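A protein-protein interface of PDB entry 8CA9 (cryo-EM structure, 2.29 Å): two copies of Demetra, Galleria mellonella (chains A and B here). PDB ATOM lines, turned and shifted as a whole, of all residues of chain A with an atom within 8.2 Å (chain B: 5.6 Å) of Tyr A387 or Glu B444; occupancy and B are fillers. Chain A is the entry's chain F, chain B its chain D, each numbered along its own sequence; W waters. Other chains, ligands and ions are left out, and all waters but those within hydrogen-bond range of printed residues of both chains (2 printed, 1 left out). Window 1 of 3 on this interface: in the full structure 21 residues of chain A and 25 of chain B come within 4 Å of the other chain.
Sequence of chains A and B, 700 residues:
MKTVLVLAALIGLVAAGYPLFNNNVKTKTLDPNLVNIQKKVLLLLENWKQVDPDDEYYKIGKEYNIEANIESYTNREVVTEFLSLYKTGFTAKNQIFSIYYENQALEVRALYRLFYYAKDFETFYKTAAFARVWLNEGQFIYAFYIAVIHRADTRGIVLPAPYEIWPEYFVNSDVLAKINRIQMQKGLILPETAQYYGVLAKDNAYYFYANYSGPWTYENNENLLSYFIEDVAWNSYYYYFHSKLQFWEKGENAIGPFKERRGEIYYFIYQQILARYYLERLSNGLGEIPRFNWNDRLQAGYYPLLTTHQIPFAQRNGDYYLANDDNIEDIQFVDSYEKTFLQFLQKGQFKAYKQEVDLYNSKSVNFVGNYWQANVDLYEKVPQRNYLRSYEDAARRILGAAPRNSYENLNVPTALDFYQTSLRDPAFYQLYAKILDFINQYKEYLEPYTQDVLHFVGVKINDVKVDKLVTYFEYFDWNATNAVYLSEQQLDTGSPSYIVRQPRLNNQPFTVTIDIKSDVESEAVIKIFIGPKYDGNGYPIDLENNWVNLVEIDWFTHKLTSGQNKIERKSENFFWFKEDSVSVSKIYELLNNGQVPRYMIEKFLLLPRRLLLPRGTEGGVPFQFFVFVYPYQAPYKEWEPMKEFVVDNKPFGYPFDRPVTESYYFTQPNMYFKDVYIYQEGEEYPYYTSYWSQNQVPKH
The side-chain hydroxyl (OH) of Tyr B445 lies within hydrogen-bond range of the backbone carbonyl oxygen (O) of Leu B345 (2.5 Å).
Water W1 lies within hydrogen-bond range of the side-chain amide oxygen (OE1) of Gln B346, the backbone carbonyl oxygen (O) of Leu B342 and the side-chain hydroxyl (OH) of Tyr A387.
Water W2 lies within hydrogen-bond range of O of Asn A386 (2.9 Å) and OE1 of Glu B444 (3.2 Å).
NH2 of Arg A385 sits at hydrogen-bond distance from O of Gln B346, at 2.7 Å.
OE1 of Glu B444 is in salt-bridge range of NH1 of Arg A389, at 3.2 Å.
The guanidinium group of Arg A385 sits at hydrogen-bond distance from the side-chain hydroxyl of Tyr B445 (3.4 Å).
No position is printed for both chains.
Printed residues of chain B that touch a printed residue of chain A: Leu B345, Gln B346, Gln B441, Glu B444, Tyr B445 and Leu B446.
Along chain B the printed residues that touch a printed residue of chain A span positions 345 to 446.
Among the printed residues, Asp or Glu carboxylates within 4 Å of a Lys or Arg side-chain nitrogen of the other chain: Arg A389 with Glu B444 (3.2 Å).
Among the printed residues, pairs that only touch across the chains: Tyr A387 with Tyr B445, Asn A386 with Glu B444, Tyr A387 with Glu B444, Tyr A387 with Gln B346, Tyr A387 with Gln B441, Asn A386 with Tyr B445, Phe A333 with Gln B346, Glu A329 with Gln B441, Asn A386 with Leu B446, Arg A389 with Gln B441 and Tyr A387 with Leu B345.
Tyr A387 touches just these residues of chain B: Leu B345, Gln B346, Gln B441, Glu B444 and Tyr B445.
Glu B444 touches just these residues of chain A: Asn A386, Tyr A387 and Arg A389.
Of the printed residues of chain A, Tyr B445 touches Arg A385 (3.4 Å), Asn A386 (3.7 Å) and Tyr A387 (3.5 Å).
Of the printed residues of chain A, Gln B441 touches Glu A329 (3.7 Å), Tyr A387 (3.7 Å) and Arg A389 (3.8 Å).
Of the printed residues of chain B, Arg A389 touches Gln B441 (3.8 Å) and Glu B444 (3.2 Å).
Of the printed residues of chain B, Glu A329 touches Gln B441.
Of the printed residues of chain B, Arg A385 touches Gln B346 and Tyr B445.
Ser A390 touches none of the printed residues of chain B.
The nearest residue of chain B that does not touch Tyr A387 is Leu B342 (4.9 Å).
The nearest printed residue of chain B that does not touch Asn A386 is Lys B443 (6.9 Å).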
ATOM      1  N   GLU A 329      23.156  12.726   0.979  1.00  0.00           N
ATOM      2  CA  GLU A 329      23.382  12.972   2.399  1.00  0.00           C
ATOM      3  C   GLU A 329      22.723  11.888   3.241  1.00  0.00           C
ATOM      4  O   GLU A 329      23.392  11.172   3.996  1.00  0.00           O
ATOM      5  CB  GLU A 329      22.851  14.353   2.787  1.00  0.00           C
ATOM      6  CG  GLU A 329      23.501  15.505   2.037  1.00  0.00           C
ATOM      7  CD  GLU A 329      23.123  16.858   2.608  1.00  0.00           C
ATOM      8  OE1 GLU A 329      22.539  16.898   3.711  1.00  0.00           O
ATOM      9  OE2 GLU A 329      23.410  17.882   1.953  1.00  0.00           O
ATOM     10  N   PHE A 333      24.420   9.011   5.851  1.00  0.00           N
ATOM     11  CA  PHE A 333      24.088   8.804   7.253  1.00  0.00           C
ATOM     12  C   PHE A 333      23.723   7.349   7.497  1.00  0.00           C
ATOM     13  O   PHE A 333      24.327   6.677   8.343  1.00  0.00           O
ATOM     14  CB  PHE A 333      22.942   9.731   7.664  1.00  0.00           C
ATOM     15  CG  PHE A 333      22.447   9.503   9.062  1.00  0.00           C
ATOM     16  CD1 PHE A 333      23.077  10.098  10.140  1.00  0.00           C
ATOM     17  CD2 PHE A 333      21.347   8.696   9.298  1.00  0.00           C
ATOM     18  CE1 PHE A 333      22.623   9.889  11.428  1.00  0.00           C
ATOM     19  CE2 PHE A 333      20.888   8.484  10.581  1.00  0.00           C
ATOM     20  CZ  PHE A 333      21.526   9.081  11.647  1.00  0.00           C
ATOM     21  N   TYR A 379      19.545   9.111  24.341  1.00  0.00           N
ATOM     22  CA  TYR A 379      20.245  10.366  24.588  1.00  0.00           C
ATOM     23  C   TYR A 379      19.955  10.938  25.973  1.00  0.00           C
ATOM     24  O   TYR A 379      20.125  12.143  26.187  1.00  0.00           O
ATOM     25  CB  TYR A 379      19.878  11.396  23.519  1.00  0.00           C
ATOM     26  CG  TYR A 379      19.969  10.889  22.098  1.00  0.00           C
ATOM     27  CD1 TYR A 379      21.191  10.809  21.444  1.00  0.00           C
ATOM     28  CD2 TYR A 379      18.830  10.500  21.407  1.00  0.00           C
ATOM     29  CE1 TYR A 379      21.275  10.349  20.144  1.00  0.00           C
ATOM     30  CE2 TYR A 379      18.905  10.041  20.107  1.00  0.00           C
ATOM     31  CZ  TYR A 379      20.129   9.968  19.480  1.00  0.00           C
ATOM     32  OH  TYR A 379      20.206   9.510  18.186  1.00  0.00           O
ATOM     33  N   PRO A 383      23.930  15.992  27.100  1.00  0.00           N
ATOM     34  CA  PRO A 383      23.177  17.247  27.191  1.00  0.00           C
ATOM     35  C   PRO A 383      22.185  17.389  26.049  1.00  0.00           C
ATOM     36  O   PRO A 383      22.378  16.852  24.955  1.00  0.00           O
ATOM     37  CB  PRO A 383      24.265  18.327  27.120  1.00  0.00           C
ATOM     38  CG  PRO A 383      25.532  17.635  27.472  1.00  0.00           C
ATOM     39  CD  PRO A 383      25.381  16.226  26.997  1.00  0.00           C
ATOM     40  N   GLN A 384      21.107  18.116  26.326  1.00  0.00           N
ATOM     41  CA  GLN A 384      20.078  18.377  25.327  1.00  0.00           C
ATOM     42  C   GLN A 384      20.707  18.826  24.016  1.00  0.00           C
ATOM     43  O   GLN A 384      21.427  19.828  23.970  1.00  0.00           O
ATOM     44  CB  GLN A 384      19.112  19.442  25.856  1.00  0.00           C
ATOM     45  CG  GLN A 384      18.051  19.909  24.865  1.00  0.00           C
ATOM     46  CD  GLN A 384      17.081  18.812  24.465  1.00  0.00           C
ATOM     47  OE1 GLN A 384      17.476  17.676  24.209  1.00  0.00           O
ATOM     48  NE2 GLN A 384      15.799  19.154  24.409  1.00  0.00           N
ATOM     49  N   ARG A 385      20.431  18.081  22.950  1.00  0.00           N
ATOM     50  CA  ARG A 385      21.023  18.325  21.644  1.00  0.00           C
ATOM     51  C   ARG A 385      20.028  19.009  20.714  1.00  0.00           C
ATOM     52  O   ARG A 385      18.833  18.706  20.718  1.00  0.00           O
ATOM     53  CB  ARG A 385      21.492  17.018  21.003  1.00  0.00           C
ATOM     54  CG  ARG A 385      22.733  16.418  21.631  1.00  0.00           C
ATOM     55  CD  ARG A 385      23.166  15.170  20.884  1.00  0.00           C
ATOM     56  NE  ARG A 385      24.374  14.580  21.445  1.00  0.00           N
ATOM     57  CZ  ARG A 385      24.927  13.455  21.011  1.00  0.00           C
ATOM     58  NH1 ARG A 385      24.407  12.772  20.005  1.00  0.00           N
ATOM     59  NH2 ARG A 385      26.030  13.005  21.603  1.00  0.00           N
ATOM     60  N   ASN A 386      20.542  19.941  19.912  1.00  0.00           N
ATOM     61  CA  ASN A 386      19.778  20.551  18.835  1.00  0.00           C
ATOM     62  C   ASN A 386      19.995  19.859  17.496  1.00  0.00           C
ATOM     63  O   ASN A 386      19.270  20.150  16.540  1.00  0.00           O
ATOM     64  CB  ASN A 386      20.139  22.035  18.702  1.00  0.00           C
ATOM     65  CG  ASN A 386      19.833  22.824  19.958  1.00  0.00           C
ATOM     66  OD1 ASN A 386      19.616  22.255  21.026  1.00  0.00           O
ATOM     67  ND2 ASN A 386      19.816  24.146  19.835  1.00  0.00           N
ATOM     68  N   TYR A 387      20.970  18.954  17.408  1.00  0.00           N
ATOM     69  CA  TYR A 387      21.235  18.181  16.200  1.00  0.00           C
ATOM     70  C   TYR A 387      20.563  16.822  16.353  1.00  0.00           C
ATOM     71  O   TYR A 387      20.991  15.997  17.167  1.00  0.00           O
ATOM     72  CB  TYR A 387      22.738  18.037  15.972  1.00  0.00           C
ATOM     73  CG  TYR A 387      23.115  17.006  14.933  1.00  0.00           C
ATOM     74  CD1 TYR A 387      23.036  17.296  13.576  1.00  0.00           C
ATOM     75  CD2 TYR A 387      23.561  15.746  15.307  1.00  0.00           C
ATOM     76  CE1 TYR A 387      23.383  16.356  12.624  1.00  0.00           C
ATOM     77  CE2 TYR A 387      23.911  14.801  14.362  1.00  0.00           C
ATOM     78  CZ  TYR A 387      23.820  15.111  13.023  1.00  0.00           C
ATOM     79  OH  TYR A 387      24.168  14.172  12.080  1.00  0.00           O
ATOM     80  N   LEU A 388      19.515  16.590  15.567  1.00  0.00           N
ATOM     81  CA  LEU A 388      18.679  15.406  15.689  1.00  0.00           C
ATOM     82  C   LEU A 388      18.693  14.623  14.384  1.00  0.00           C
ATOM     83  O   LEU A 388      18.547  15.199  13.300  1.00  0.00           O
ATOM     84  CB  LEU A 388      17.239  15.792  16.046  1.00  0.00           C
ATOM     85  CG  LEU A 388      17.069  16.754  17.224  1.00  0.00           C
ATOM     86  CD1 LEU A 388      15.692  17.400  17.191  1.00  0.00           C
ATOM     87  CD2 LEU A 388      17.293  16.039  18.547  1.00  0.00           C
ATOM     88  N   ARG A 389      18.869  13.307  14.492  1.00  0.00           N
ATOM     89  CA  ARG A 389      18.832  12.425  13.336  1.00  0.00           C
ATOM     90  C   ARG A 389      18.248  11.085  13.757  1.00  0.00           C
ATOM     91  O   ARG A 389      18.337  10.691  14.923  1.00  0.00           O
ATOM     92  CB  ARG A 389      20.226  12.226  12.727  1.00  0.00           C
ATOM     93  CG  ARG A 389      20.801  13.461  12.049  1.00  0.00           C
ATOM     94  CD  ARG A 389      19.999  13.847  10.816  1.00  0.00           C
ATOM     95  NE  ARG A 389      20.638  14.913  10.053  1.00  0.00           N
ATOM     96  CZ  ARG A 389      20.470  16.210  10.278  1.00  0.00           C
ATOM     97  NH1 ARG A 389      19.691  16.650  11.253  1.00  0.00           N
ATOM     98  NH2 ARG A 389      21.104  17.088   9.507  1.00  0.00           N
ATOM     99  N   SER A 390      17.647  10.388  12.793  1.00  0.00           N
ATOM    100  CA  SER A 390      17.029   9.093  13.039  1.00  0.00           C
ATOM    101  C   SER A 390      17.281   8.178  11.852  1.00  0.00           C
ATOM    102  O   SER A 390      17.017   8.555  10.706  1.00  0.00           O
ATOM    103  CB  SER A 390      15.522   9.239  13.283  1.00  0.00           C
ATOM    104  OG  SER A 390      14.899   7.974  13.407  1.00  0.00           O
ATOM    105  N   LEU B 342      30.865  12.375  10.519  1.00  0.00           N
ATOM    106  CA  LEU B 342      29.512  12.061  10.957  1.00  0.00           C
ATOM    107  C   LEU B 342      29.530  11.404  12.330  1.00  0.00           C
ATOM    108  O   LEU B 342      28.729  11.754  13.205  1.00  0.00           O
ATOM    109  CB  LEU B 342      28.823  11.160   9.932  1.00  0.00           C
ATOM    110  CG  LEU B 342      28.523  11.807   8.577  1.00  0.00           C
ATOM    111  CD1 LEU B 342      28.025  10.774   7.580  1.00  0.00           C
ATOM    112  CD2 LEU B 342      27.510  12.932   8.726  1.00  0.00           C
ATOM    113  N   LEU B 345      29.743  13.864  14.980  1.00  0.00           N
ATOM    114  CA  LEU B 345      28.470  14.532  15.229  1.00  0.00           C
ATOM    115  C   LEU B 345      27.607  13.722  16.187  1.00  0.00           C
ATOM    116  O   LEU B 345      26.831  14.288  16.964  1.00  0.00           O
ATOM    117  CB  LEU B 345      27.737  14.775  13.911  1.00  0.00           C
ATOM    118  CG  LEU B 345      28.477  15.628  12.877  1.00  0.00           C
ATOM    119  CD1 LEU B 345      27.639  15.794  11.621  1.00  0.00           C
ATOM    120  CD2 LEU B 345      28.850  16.985  13.453  1.00  0.00           C
ATOM    121  N   GLN B 346      27.725  12.392  16.144  1.00  0.00           N
ATOM    122  CA  GLN B 346      26.972  11.566  17.079  1.00  0.00           C
ATOM    123  C   GLN B 346      27.575  11.612  18.477  1.00  0.00           C
ATOM    124  O   GLN B 346      26.839  11.537  19.469  1.00  0.00           O
ATOM    125  CB  GLN B 346      26.910  10.123  16.574  1.00  0.00           C
ATOM    126  CG  GLN B 346      26.253   9.968  15.211  1.00  0.00           C
ATOM    127  CD  GLN B 346      24.806  10.421  15.197  1.00  0.00           C
ATOM    128  OE1 GLN B 346      24.403  11.219  14.352  1.00  0.00           O
ATOM    129  NE2 GLN B 346      24.014   9.908  16.131  1.00  0.00           N
ATOM    130  N   ILE B 439      29.653  21.123   7.181  1.00  0.00           N
ATOM    131  CA  ILE B 439      29.924  22.095   8.236  1.00  0.00           C
ATOM    132  C   ILE B 439      28.628  22.676   8.790  1.00  0.00           C
ATOM    133  O   ILE B 439      28.536  22.966   9.986  1.00  0.00           O
ATOM    134  CB  ILE B 439      30.874  23.199   7.728  1.00  0.00           C
ATOM    135  CG1 ILE B 439      32.232  22.586   7.369  1.00  0.00           C
ATOM    136  CG2 ILE B 439      31.045  24.280   8.789  1.00  0.00           C
ATOM    137  CD1 ILE B 439      33.248  23.575   6.834  1.00  0.00           C
ATOM    138  N   ASN B 440      27.610  22.857   7.948  1.00  0.00           N
ATOM    139  CA  ASN B 440      26.326  23.356   8.439  1.00  0.00           C
ATOM    140  C   ASN B 440      25.598  22.295   9.255  1.00  0.00           C
ATOM    141  O   ASN B 440      24.914  22.613  10.236  1.00  0.00           O
ATOM    142  CB  ASN B 440      25.464  23.825   7.269  1.00  0.00           C
ATOM    143  CG  ASN B 440      26.012  25.072   6.605  1.00  0.00           C
ATOM    144  OD1 ASN B 440      26.547  25.960   7.269  1.00  0.00           O
ATOM    145  ND2 ASN B 440      25.885  25.141   5.288  1.00  0.00           N
ATOM    146  N   GLN B 441      25.724  21.026   8.861  1.00  0.00           N
ATOM    147  CA  GLN B 441      25.230  19.951   9.716  1.00  0.00           C
ATOM    148  C   GLN B 441      25.857  20.049  11.100  1.00  0.00           C
ATOM    149  O   GLN B 441      25.173  19.878  12.117  1.00  0.00           O
ATOM    150  CB  GLN B 441      25.528  18.588   9.089  1.00  0.00           C
ATOM    151  CG  GLN B 441      24.665  18.240   7.883  1.00  0.00           C
ATOM    152  CD  GLN B 441      24.802  16.786   7.477  1.00  0.00           C
ATOM    153  OE1 GLN B 441      25.103  16.475   6.324  1.00  0.00           O
ATOM    154  NE2 GLN B 441      24.574  15.882   8.425  1.00  0.00           N
ATOM    155  N   TYR B 442      27.162  20.323  11.154  1.00  0.00           N
ATOM    156  CA  TYR B 442      27.799  20.595  12.440  1.00  0.00           C
ATOM    157  C   TYR B 442      27.186  21.816  13.121  1.00  0.00           C
ATOM    158  O   TYR B 442      26.899  21.788  14.324  1.00  0.00           O
ATOM    159  CB  TYR B 442      29.298  20.815  12.261  1.00  0.00           C
ATOM    160  CG  TYR B 442      29.838  21.865  13.205  1.00  0.00           C
ATOM    161  CD1 TYR B 442      29.970  21.603  14.561  1.00  0.00           C
ATOM    162  CD2 TYR B 442      30.196  23.123  12.743  1.00  0.00           C
ATOM    163  CE1 TYR B 442      30.449  22.559  15.427  1.00  0.00           C
ATOM    164  CE2 TYR B 442      30.680  24.085  13.603  1.00  0.00           C
ATOM    165  CZ  TYR B 442      30.805  23.797  14.944  1.00  0.00           C
ATOM    166  OH  TYR B 442      31.286  24.753  15.808  1.00  0.00           O
ATOM    167  N   LYS B 443      26.997  22.903  12.370  1.00  0.00           N
ATOM    168  CA  LYS B 443      26.486  24.148  12.930  1.00  0.00           C
ATOM    169  C   LYS B 443      25.103  23.985  13.533  1.00  0.00           C
ATOM    170  O   LYS B 443      24.706  24.793  14.379  1.00  0.00           O
ATOM    171  CB  LYS B 443      26.425  25.225  11.849  1.00  0.00           C
ATOM    172  CG  LYS B 443      27.757  25.793  11.423  1.00  0.00           C
ATOM    173  CD  LYS B 443      28.382  26.625  12.528  1.00  0.00           C
ATOM    174  CE  LYS B 443      29.633  27.342  12.053  1.00  0.00           C
ATOM    175  NZ  LYS B 443      29.325  28.362  11.016  1.00  0.00           N
ATOM    176  N   GLU B 444      24.357  22.972  13.098  1.00  0.00           N
ATOM    177  CA  GLU B 444      23.035  22.737  13.668  1.00  0.00           C
ATOM    178  C   GLU B 444      23.093  22.559  15.180  1.00  0.00           C
ATOM    179  O   GLU B 444      22.091  22.798  15.862  1.00  0.00           O
ATOM    180  CB  GLU B 444      22.395  21.501  13.031  1.00  0.00           C
ATOM    181  CG  GLU B 444      22.035  21.656  11.565  1.00  0.00           C
ATOM    182  CD  GLU B 444      21.311  20.441  11.012  1.00  0.00           C
ATOM    183  OE1 GLU B 444      20.937  19.555  11.811  1.00  0.00           O
ATOM    184  OE2 GLU B 444      21.115  20.371   9.781  1.00  0.00           O
ATOM    185  N   TYR B 445      24.246  22.147  15.715  1.00  0.00           N
ATOM    186  CA  TYR B 445      24.391  21.988  17.159  1.00  0.00           C
ATOM    187  C   TYR B 445      24.180  23.300  17.903  1.00  0.00           C
ATOM    188  O   TYR B 445      23.566  23.313  18.975  1.00  0.00           O
ATOM    189  CB  TYR B 445      25.782  21.440  17.484  1.00  0.00           C
ATOM    190  CG  TYR B 445      25.823  19.965  17.808  1.00  0.00           C
ATOM    191  CD1 TYR B 445      25.947  19.016  16.803  1.00  0.00           C
ATOM    192  CD2 TYR B 445      25.753  19.524  19.120  1.00  0.00           C
ATOM    193  CE1 TYR B 445      25.993  17.668  17.098  1.00  0.00           C
ATOM    194  CE2 TYR B 445      25.796  18.178  19.425  1.00  0.00           C
ATOM    195  CZ  TYR B 445      25.916  17.255  18.411  1.00  0.00           C
ATOM    196  OH  TYR B 445      25.961  15.913  18.712  1.00  0.00           O
ATOM    197  N   LEU B 446      24.681  24.405  17.357  1.00  0.00           N
ATOM    198  CA  LEU B 446      24.762  25.649  18.110  1.00  0.00           C
ATOM    199  C   LEU B 446      23.379  26.176  18.478  1.00  0.00           C
ATOM    200  O   LEU B 446      22.406  26.019  17.734  1.00  0.00           O
ATOM    201  CB  LEU B 446      25.517  26.705  17.303  1.00  0.00           C
ATOM    202  CG  LEU B 446      26.919  26.294  16.850  1.00  0.00           C
ATOM    203  CD1 LEU B 446      27.552  27.380  15.996  1.00  0.00           C
ATOM    204  CD2 LEU B 446      27.803  25.966  18.043  1.00  0.00           C
ATOM    205  N   PRO B 659      22.754  28.896  12.272  1.00  0.00           N
ATOM    206  CA  PRO B 659      21.456  28.748  11.601  1.00  0.00           C
ATOM    207  C   PRO B 659      20.365  29.576  12.264  1.00  0.00           C
ATOM    208  O   PRO B 659      20.347  29.758  13.483  1.00  0.00           O
ATOM    209  CB  PRO B 659      21.163  27.247  11.714  1.00  0.00           C
ATOM    210  CG  PRO B 659      22.470  26.607  12.017  1.00  0.00           C
ATOM    211  CD  PRO B 659      23.252  27.613  12.793  1.00  0.00           C
HETATM  212  O   HOH W   1      25.827  11.366  12.187  1.00  0.00           O
HETATM  213  O   HOH W   2      18.393  19.598  13.797  1.00  0.00           O
